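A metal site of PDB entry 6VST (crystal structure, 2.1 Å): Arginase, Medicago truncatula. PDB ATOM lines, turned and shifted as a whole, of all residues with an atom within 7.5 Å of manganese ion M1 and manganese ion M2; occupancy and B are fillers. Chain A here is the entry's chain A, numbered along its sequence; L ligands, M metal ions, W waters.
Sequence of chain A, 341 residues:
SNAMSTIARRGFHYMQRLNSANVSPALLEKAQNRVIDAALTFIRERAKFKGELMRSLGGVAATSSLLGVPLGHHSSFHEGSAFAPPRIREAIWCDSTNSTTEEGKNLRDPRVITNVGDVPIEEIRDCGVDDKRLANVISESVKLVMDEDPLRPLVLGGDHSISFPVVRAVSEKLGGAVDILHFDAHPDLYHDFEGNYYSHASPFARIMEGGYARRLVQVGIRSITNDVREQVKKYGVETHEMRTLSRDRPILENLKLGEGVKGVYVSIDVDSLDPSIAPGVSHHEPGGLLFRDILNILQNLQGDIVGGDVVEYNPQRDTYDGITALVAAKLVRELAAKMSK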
ATOM      1  N   ASP A 159      36.827  -6.192  17.137  1.00  0.00           N
ATOM      2  CA  ASP A 159      35.491  -6.515  17.640  1.00  0.00           C
ATOM      3  C   ASP A 159      35.224  -5.706  18.903  1.00  0.00           C
ATOM      4  O   ASP A 159      36.101  -5.014  19.448  1.00  0.00           O
ATOM      5  CB  ASP A 159      35.313  -8.028  17.878  1.00  0.00           C
ATOM      6  CG  ASP A 159      36.245  -8.605  18.948  1.00  0.00           C
ATOM      7  OD1 ASP A 159      36.361  -8.010  20.055  1.00  0.00           O
ATOM      8  OD2 ASP A 159      36.825  -9.688  18.696  1.00  0.00           O
ATOM      9  N   HIS A 160      33.982  -5.795  19.393  1.00  0.00           N
ATOM     10  CA  HIS A 160      33.571  -4.860  20.432  1.00  0.00           C
ATOM     11  C   HIS A 160      34.219  -5.141  21.801  1.00  0.00           C
ATOM     12  O   HIS A 160      34.055  -4.333  22.712  1.00  0.00           O
ATOM     13  CB  HIS A 160      32.042  -4.862  20.563  1.00  0.00           C
ATOM     14  CG  HIS A 160      31.485  -3.509  20.870  1.00  0.00           C
ATOM     15  ND1 HIS A 160      30.222  -3.119  20.496  1.00  0.00           N
ATOM     16  CD2 HIS A 160      32.050  -2.428  21.476  1.00  0.00           C
ATOM     17  CE1 HIS A 160      30.015  -1.868  20.868  1.00  0.00           C
ATOM     18  NE2 HIS A 160      31.108  -1.425  21.465  1.00  0.00           N
ATOM     19  N   SER A 161      34.911  -6.270  21.975  1.00  0.00           N
ATOM     20  CA  SER A 161      35.591  -6.545  23.246  1.00  0.00           C
ATOM     21  C   SER A 161      36.577  -5.453  23.610  1.00  0.00           C
ATOM     22  O   SER A 161      36.847  -5.224  24.796  1.00  0.00           O
ATOM     23  CB  SER A 161      36.313  -7.883  23.190  1.00  0.00           C
ATOM     24  OG  SER A 161      37.436  -7.834  22.312  1.00  0.00           O
ATOM     25  N   SER A 163      36.254  -2.328  23.661  1.00  0.00           N
ATOM     26  CA  SER A 163      35.757  -1.162  24.385  1.00  0.00           C
ATOM     27  C   SER A 163      36.053  -1.252  25.885  1.00  0.00           C
ATOM     28  O   SER A 163      36.217  -0.226  26.554  1.00  0.00           O
ATOM     29  CB  SER A 163      34.253  -1.016  24.138  1.00  0.00           C
ATOM     30  OG  SER A 163      34.007  -0.515  22.843  1.00  0.00           O
ATOM     31  N   HIS A 182      26.279   4.646  23.434  1.00  0.00           N
ATOM     32  CA  HIS A 182      26.621   3.346  22.859  1.00  0.00           C
ATOM     33  C   HIS A 182      25.587   2.998  21.782  1.00  0.00           C
ATOM     34  O   HIS A 182      24.397   2.824  22.094  1.00  0.00           O
ATOM     35  CB  HIS A 182      26.655   2.298  23.974  1.00  0.00           C
ATOM     36  CG  HIS A 182      26.818   0.882  23.510  1.00  0.00           C
ATOM     37  ND1 HIS A 182      26.279  -0.175  24.193  1.00  0.00           N
ATOM     38  CD2 HIS A 182      27.490   0.349  22.460  1.00  0.00           C
ATOM     39  CE1 HIS A 182      26.599  -1.312  23.584  1.00  0.00           C
ATOM     40  NE2 HIS A 182      27.364  -1.012  22.547  1.00  0.00           N
ATOM     41  N   PHE A 183      26.037   2.923  20.529  1.00  0.00           N
ATOM     42  CA  PHE A 183      25.198   2.519  19.399  1.00  0.00           C
ATOM     43  C   PHE A 183      25.453   1.056  19.086  1.00  0.00           C
ATOM     44  O   PHE A 183      26.600   0.658  18.826  1.00  0.00           O
ATOM     45  CB  PHE A 183      25.505   3.336  18.129  1.00  0.00           C
ATOM     46  CG  PHE A 183      25.229   4.811  18.269  1.00  0.00           C
ATOM     47  CD1 PHE A 183      23.964   5.320  18.017  1.00  0.00           C
ATOM     48  CD2 PHE A 183      26.242   5.681  18.624  1.00  0.00           C
ATOM     49  CE1 PHE A 183      23.698   6.673  18.133  1.00  0.00           C
ATOM     50  CE2 PHE A 183      25.984   7.054  18.733  1.00  0.00           C
ATOM     51  CZ  PHE A 183      24.718   7.548  18.484  1.00  0.00           C
ATOM     52  N   ASP A 184      24.384   0.262  19.048  1.00  0.00           N
ATOM     53  CA  ASP A 184      24.582  -1.167  18.911  1.00  0.00           C
ATOM     54  C   ASP A 184      23.241  -1.843  18.639  1.00  0.00           C
ATOM     55  O   ASP A 184      22.190  -1.366  19.100  1.00  0.00           O
ATOM     56  CB  ASP A 184      25.229  -1.742  20.182  1.00  0.00           C
ATOM     57  CG  ASP A 184      26.137  -2.922  19.901  1.00  0.00           C
ATOM     58  OD1 ASP A 184      25.731  -3.767  19.076  1.00  0.00           O
ATOM     59  OD2 ASP A 184      27.258  -2.964  20.479  1.00  0.00           O
ATOM     60  N   ALA A 185      23.273  -2.936  17.860  1.00  0.00           N
ATOM     61  CA  ALA A 185      22.126  -3.838  17.810  1.00  0.00           C
ATOM     62  C   ALA A 185      21.995  -4.663  19.077  1.00  0.00           C
ATOM     63  O   ALA A 185      20.901  -5.180  19.360  1.00  0.00           O
ATOM     64  CB  ALA A 185      22.237  -4.775  16.613  1.00  0.00           C
ATOM     65  N   HIS A 186      23.086  -4.803  19.843  1.00  0.00           N
ATOM     66  CA  HIS A 186      23.235  -5.698  20.991  1.00  0.00           C
ATOM     67  C   HIS A 186      23.675  -4.935  22.232  1.00  0.00           C
ATOM     68  O   HIS A 186      24.597  -4.115  22.163  1.00  0.00           O
ATOM     69  CB  HIS A 186      24.261  -6.812  20.707  1.00  0.00           C
ATOM     70  CG  HIS A 186      24.121  -7.426  19.340  1.00  0.00           C
ATOM     71  ND1 HIS A 186      24.810  -6.978  18.233  1.00  0.00           N
ATOM     72  CD2 HIS A 186      23.354  -8.471  18.909  1.00  0.00           C
ATOM     73  CE1 HIS A 186      24.498  -7.713  17.182  1.00  0.00           C
ATOM     74  NE2 HIS A 186      23.610  -8.627  17.565  1.00  0.00           N
ATOM     75  N   PRO A 187      23.081  -5.224  23.393  1.00  0.00           N
ATOM     76  CA  PRO A 187      23.492  -4.538  24.626  1.00  0.00           C
ATOM     77  C   PRO A 187      24.916  -4.845  25.040  1.00  0.00           C
ATOM     78  O   PRO A 187      25.501  -4.028  25.749  1.00  0.00           O
ATOM     79  CB  PRO A 187      22.490  -5.055  25.672  1.00  0.00           C
ATOM     80  CG  PRO A 187      21.325  -5.598  24.818  1.00  0.00           C
ATOM     81  CD  PRO A 187      22.012  -6.205  23.655  1.00  0.00           C
ATOM     82  N   ASP A 188      25.486  -5.992  24.607  1.00  0.00           N
ATOM     83  CA  ASP A 188      26.849  -6.411  24.965  1.00  0.00           C
ATOM     84  C   ASP A 188      27.051  -6.421  26.483  1.00  0.00           C
ATOM     85  O   ASP A 188      28.084  -5.986  26.999  1.00  0.00           O
ATOM     86  CB  ASP A 188      27.898  -5.522  24.292  1.00  0.00           C
ATOM     87  CG  ASP A 188      27.959  -5.718  22.773  1.00  0.00           C
ATOM     88  OD1 ASP A 188      27.378  -6.698  22.266  1.00  0.00           O
ATOM     89  OD2 ASP A 188      28.608  -4.896  22.107  1.00  0.00           O
ATOM     90  N   HIS A 200      33.302 -10.362  22.994  1.00  0.00           N
ATOM     91  CA  HIS A 200      32.781  -9.110  22.437  1.00  0.00           C
ATOM     92  C   HIS A 200      31.317  -8.879  22.799  1.00  0.00           C
ATOM     93  O   HIS A 200      30.793  -7.802  22.530  1.00  0.00           O
ATOM     94  CB  HIS A 200      32.959  -9.069  20.904  1.00  0.00           C
ATOM     95  CG  HIS A 200      32.052  -9.997  20.132  1.00  0.00           C
ATOM     96  ND1 HIS A 200      31.619  -9.717  18.853  1.00  0.00           N
ATOM     97  CD2 HIS A 200      31.522 -11.208  20.440  1.00  0.00           C
ATOM     98  CE1 HIS A 200      30.853 -10.699  18.412  1.00  0.00           C
ATOM     99  NE2 HIS A 200      30.793 -11.624  19.356  1.00  0.00           N
ATOM    100  N   ALA A 201      30.654  -9.870  23.368  1.00  0.00           N
ATOM    101  CA  ALA A 201      29.283  -9.737  23.842  1.00  0.00           C
ATOM    102  C   ALA A 201      29.217  -9.313  25.299  1.00  0.00           C
ATOM    103  O   ALA A 201      28.119  -9.212  25.847  1.00  0.00           O
ATOM    104  CB  ALA A 201      28.517 -11.049  23.639  1.00  0.00           C
ATOM    105  N   PRO A 203      31.720  -6.580  26.813  1.00  0.00           N
ATOM    106  CA  PRO A 203      32.551  -5.459  27.304  1.00  0.00           C
ATOM    107  C   PRO A 203      31.785  -4.460  28.160  1.00  0.00           C
ATOM    108  O   PRO A 203      32.402  -3.813  29.023  1.00  0.00           O
ATOM    109  CB  PRO A 203      33.046  -4.792  26.009  1.00  0.00           C
ATOM    110  CG  PRO A 203      31.876  -5.079  25.020  1.00  0.00           C
ATOM    111  CD  PRO A 203      31.531  -6.490  25.347  1.00  0.00           C
ATOM    112  N   PHE A 204      30.473  -4.311  27.970  1.00  0.00           N
ATOM    113  CA  PHE A 204      29.796  -3.334  28.804  1.00  0.00           C
ATOM    114  C   PHE A 204      29.371  -3.928  30.142  1.00  0.00           C
ATOM    115  O   PHE A 204      29.211  -3.167  31.114  1.00  0.00           O
ATOM    116  CB  PHE A 204      28.632  -2.698  28.046  1.00  0.00           C
ATOM    117  CG  PHE A 204      29.122  -1.807  26.931  1.00  0.00           C
ATOM    118  CD1 PHE A 204      29.503  -0.493  27.204  1.00  0.00           C
ATOM    119  CD2 PHE A 204      29.346  -2.328  25.664  1.00  0.00           C
ATOM    120  CE1 PHE A 204      30.029   0.313  26.195  1.00  0.00           C
ATOM    121  CE2 PHE A 204      29.884  -1.525  24.649  1.00  0.00           C
ATOM    122  CZ  PHE A 204      30.219  -0.205  24.924  1.00  0.00           C
ATOM    123  N   ILE A 221      19.039  -0.961  19.872  1.00  0.00           N
ATOM    124  CA  ILE A 221      18.988  -2.320  20.387  1.00  0.00           C
ATOM    125  C   ILE A 221      17.781  -3.062  19.822  1.00  0.00           C
ATOM    126  O   ILE A 221      16.641  -2.589  19.874  1.00  0.00           O
ATOM    127  CB  ILE A 221      18.953  -2.318  21.929  1.00  0.00           C
ATOM    128  CG1 ILE A 221      20.208  -1.608  22.507  1.00  0.00           C
ATOM    129  CG2 ILE A 221      18.797  -3.744  22.441  1.00  0.00           C
ATOM    130  CD1 ILE A 221      21.488  -2.341  22.287  1.00  0.00           C
ATOM    131  N   SER A 267      30.783   4.914  21.886  1.00  0.00           N
ATOM    132  CA  SER A 267      31.117   3.633  21.255  1.00  0.00           C
ATOM    133  C   SER A 267      30.118   3.353  20.139  1.00  0.00           C
ATOM    134  O   SER A 267      28.906   3.277  20.382  1.00  0.00           O
ATOM    135  CB  SER A 267      31.133   2.487  22.267  1.00  0.00           C
ATOM    136  OG  SER A 267      31.463   1.221  21.670  1.00  0.00           O
ATOM    137  N   ILE A 268      30.616   3.206  18.915  1.00  0.00           N
ATOM    138  CA  ILE A 268      29.770   3.025  17.737  1.00  0.00           C
ATOM    139  C   ILE A 268      30.043   1.642  17.175  1.00  0.00           C
ATOM    140  O   ILE A 268      31.096   1.404  16.567  1.00  0.00           O
ATOM    141  CB  ILE A 268      30.001   4.101  16.669  1.00  0.00           C
ATOM    142  CG1 ILE A 268      30.067   5.482  17.311  1.00  0.00           C
ATOM    143  CG2 ILE A 268      28.886   4.016  15.590  1.00  0.00           C
ATOM    144  CD1 ILE A 268      30.133   6.642  16.310  1.00  0.00           C
ATOM    145  N   ASP A 269      29.095   0.718  17.363  1.00  0.00           N
ATOM    146  CA  ASP A 269      29.167  -0.588  16.740  1.00  0.00           C
ATOM    147  C   ASP A 269      28.496  -0.492  15.374  1.00  0.00           C
ATOM    148  O   ASP A 269      27.312  -0.127  15.292  1.00  0.00           O
ATOM    149  CB  ASP A 269      28.506  -1.639  17.637  1.00  0.00           C
ATOM    150  CG  ASP A 269      28.611  -3.059  17.079  1.00  0.00           C
ATOM    151  OD1 ASP A 269      28.668  -3.259  15.838  1.00  0.00           O
ATOM    152  OD2 ASP A 269      28.649  -3.982  17.912  1.00  0.00           O
ATOM    153  N   VAL A 270      29.233  -0.797  14.305  1.00  0.00           N
ATOM    154  CA  VAL A 270      28.681  -0.640  12.957  1.00  0.00           C
ATOM    155  C   VAL A 270      27.444  -1.522  12.770  1.00  0.00           C
ATOM    156  O   VAL A 270      26.574  -1.183  11.972  1.00  0.00           O
ATOM    157  CB  VAL A 270      29.775  -0.894  11.883  1.00  0.00           C
ATOM    158  CG1 VAL A 270      29.197  -0.821  10.457  1.00  0.00           C
ATOM    159  CG2 VAL A 270      30.909   0.154  12.001  1.00  0.00           C
ATOM    160  N   ASP A 271      27.278  -2.609  13.529  1.00  0.00           N
ATOM    161  CA  ASP A 271      26.075  -3.414  13.313  1.00  0.00           C
ATOM    162  C   ASP A 271      24.817  -2.789  13.924  1.00  0.00           C
ATOM    163  O   ASP A 271      23.733  -3.388  13.835  1.00  0.00           O
ATOM    164  CB  ASP A 271      26.291  -4.847  13.797  1.00  0.00           C
ATOM    165  CG  ASP A 271      26.273  -5.012  15.316  1.00  0.00           C
ATOM    166  OD1 ASP A 271      25.750  -4.157  16.060  1.00  0.00           O
ATOM    167  OD2 ASP A 271      26.800  -6.063  15.752  1.00  0.00           O
ATOM    168  N   SER A 272      24.922  -1.607  14.537  1.00  0.00           N
ATOM    169  CA  SER A 272      23.722  -0.864  14.895  1.00  0.00           C
ATOM    170  C   SER A 272      22.953  -0.435  13.653  1.00  0.00           C
ATOM    171  O   SER A 272      21.722  -0.332  13.688  1.00  0.00           O
ATOM    172  CB  SER A 272      24.077   0.341  15.747  1.00  0.00           C
ATOM    173  OG  SER A 272      24.920   1.249  15.045  1.00  0.00           O
ATOM    174  N   HIS A 283      27.444  -9.722  12.689  1.00  0.00           N
ATOM    175  CA  HIS A 283      26.109 -10.012  13.210  1.00  0.00           C
ATOM    176  C   HIS A 283      25.057  -9.168  12.502  1.00  0.00           C
ATOM    177  O   HIS A 283      24.731  -8.053  12.921  1.00  0.00           O
ATOM    178  CB  HIS A 283      26.085  -9.824  14.710  1.00  0.00           C
ATOM    179  CG  HIS A 283      27.038 -10.752  15.403  1.00  0.00           C
ATOM    180  ND1 HIS A 283      26.691 -12.045  15.738  1.00  0.00           N
ATOM    181  CD2 HIS A 283      28.340 -10.621  15.722  1.00  0.00           C
ATOM    182  CE1 HIS A 283      27.730 -12.652  16.273  1.00  0.00           C
ATOM    183  NE2 HIS A 283      28.746 -11.810  16.265  1.00  0.00           N
ATOM    184  N   VAL A 311      33.652   0.139  15.966  1.00  0.00           N
ATOM    185  CA  VAL A 311      34.001  -1.278  16.055  1.00  0.00           C
ATOM    186  C   VAL A 311      33.096  -2.115  15.155  1.00  0.00           C
ATOM    187  O   VAL A 311      32.024  -1.686  14.729  1.00  0.00           O
ATOM    188  CB  VAL A 311      33.946  -1.805  17.516  1.00  0.00           C
ATOM    189  CG1 VAL A 311      34.869  -0.996  18.432  1.00  0.00           C
ATOM    190  CG2 VAL A 311      32.506  -1.803  18.055  1.00  0.00           C
ATOM    191  N   GLU A 312      33.565  -3.341  14.890  1.00  0.00           N
ATOM    192  CA  GLU A 312      32.851  -4.456  14.278  1.00  0.00           C
ATOM    193  C   GLU A 312      32.673  -4.302  12.774  1.00  0.00           C
ATOM    194  O   GLU A 312      31.961  -5.107  12.190  1.00  0.00           O
ATOM    195  CB  GLU A 312      31.483  -4.733  14.918  1.00  0.00           C
ATOM    196  CG  GLU A 312      31.536  -5.196  16.404  1.00  0.00           C
ATOM    197  CD  GLU A 312      31.797  -6.696  16.609  1.00  0.00           C
ATOM    198  OE1 GLU A 312      31.604  -7.528  15.689  1.00  0.00           O
ATOM    199  OE2 GLU A 312      32.177  -7.063  17.744  1.00  0.00           O
HETATM  200  N1  LIG L   1      24.933 -13.393  19.489  1.00  0.00           N
HETATM  201  C1  LIG L   1      25.413 -12.258  20.316  1.00  0.00           C
HETATM  202  C2  LIG L   1      26.020 -11.180  19.411  1.00  0.00           C
HETATM  203  C3  LIG L   1      27.053 -10.267  20.071  1.00  0.00           C
HETATM  204  C4  LIG L   1      27.691  -9.297  19.083  1.00  0.00           C
HETATM  205  N2  LIG L   1      28.593  -8.275  19.628  1.00  0.00           N
HETATM  206  C5  LIG L   1      24.240 -11.740  21.170  1.00  0.00           C
HETATM  207  O1  LIG L   1      23.468 -12.607  21.679  1.00  0.00           O
HETATM  208  O2  LIG L   1      24.128 -10.500  21.320  1.00  0.00           O
HETATM  209 MN    MN M   1      28.603  -4.331  20.135  1.00  0.00          MN
HETATM  210 MN    MN M   2      26.613  -5.401  17.977  1.00  0.00          MN
HETATM  211  O   HOH W   1      28.147  -6.002  19.663  1.00  0.00           O
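Manganese ion M1 is bound by water W1 (1.8 Å), the side-chain carboxylate (OD2) of Asp 184 (1.9 Å), the side-chain carboxylate (OD2) of Asp 188 (2.1 Å), a ring nitrogen (ND1) of His 160 (2.1 Å) and the side-chain carboxylate (OD2) of Asp 269 (2.3 Å).
Within 4 Å of manganese ion M1: His 160, Asp 184, Asp 188 and Asp 269.
Manganese ion M2 is bound by OD1 of Asp 184 (2.2 Å), OD2 of Asp 271 (2.3 Å), water W1 (2.4 Å), ND1 of His 186 (2.4 Å), OD1 of Asp 271 (2.4 Å) and OD2 of Asp 269 (2.5 Å).
OD2 of Asp 184 sits close to NE2 of His 182 (2.8 Å). The backbone carbonyl oxygen of Asp 184 is in hydrogen-bond range of the backbone NH of Ile 221 (3.3 Å). O of Asp 188 lies within hydrogen-bond range of N of Phe 204, 3.1 Å away. The backbone NH of His 160 is in hydrogen-bond range of the side-chain carboxylate of Glu 312. NE2 of His 160 is in hydrogen-bond range of OG of Ser 267 (2.7 Å). NE2 of His 160 sits close to OG of Ser 163, at 3.3 Å. OG of Ser 272 sits at hydrogen-bond distance from O of Asp 269, at 2.8 Å. OD1 of Asp 271 sits close to N of Ala 185.
Four residues have an atom within 4 Å of manganese ion M2: Asp 184, His 186, Asp 269 and Asp 271.
The side-chain carboxylate (OD1) of Asp 188 is in salt-bridge range of a nitrogen (N2) of the ligand, at 3.3 Å. ND1 of His 200 is in hydrogen-bond range of N2 of the ligand (3.4 Å).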
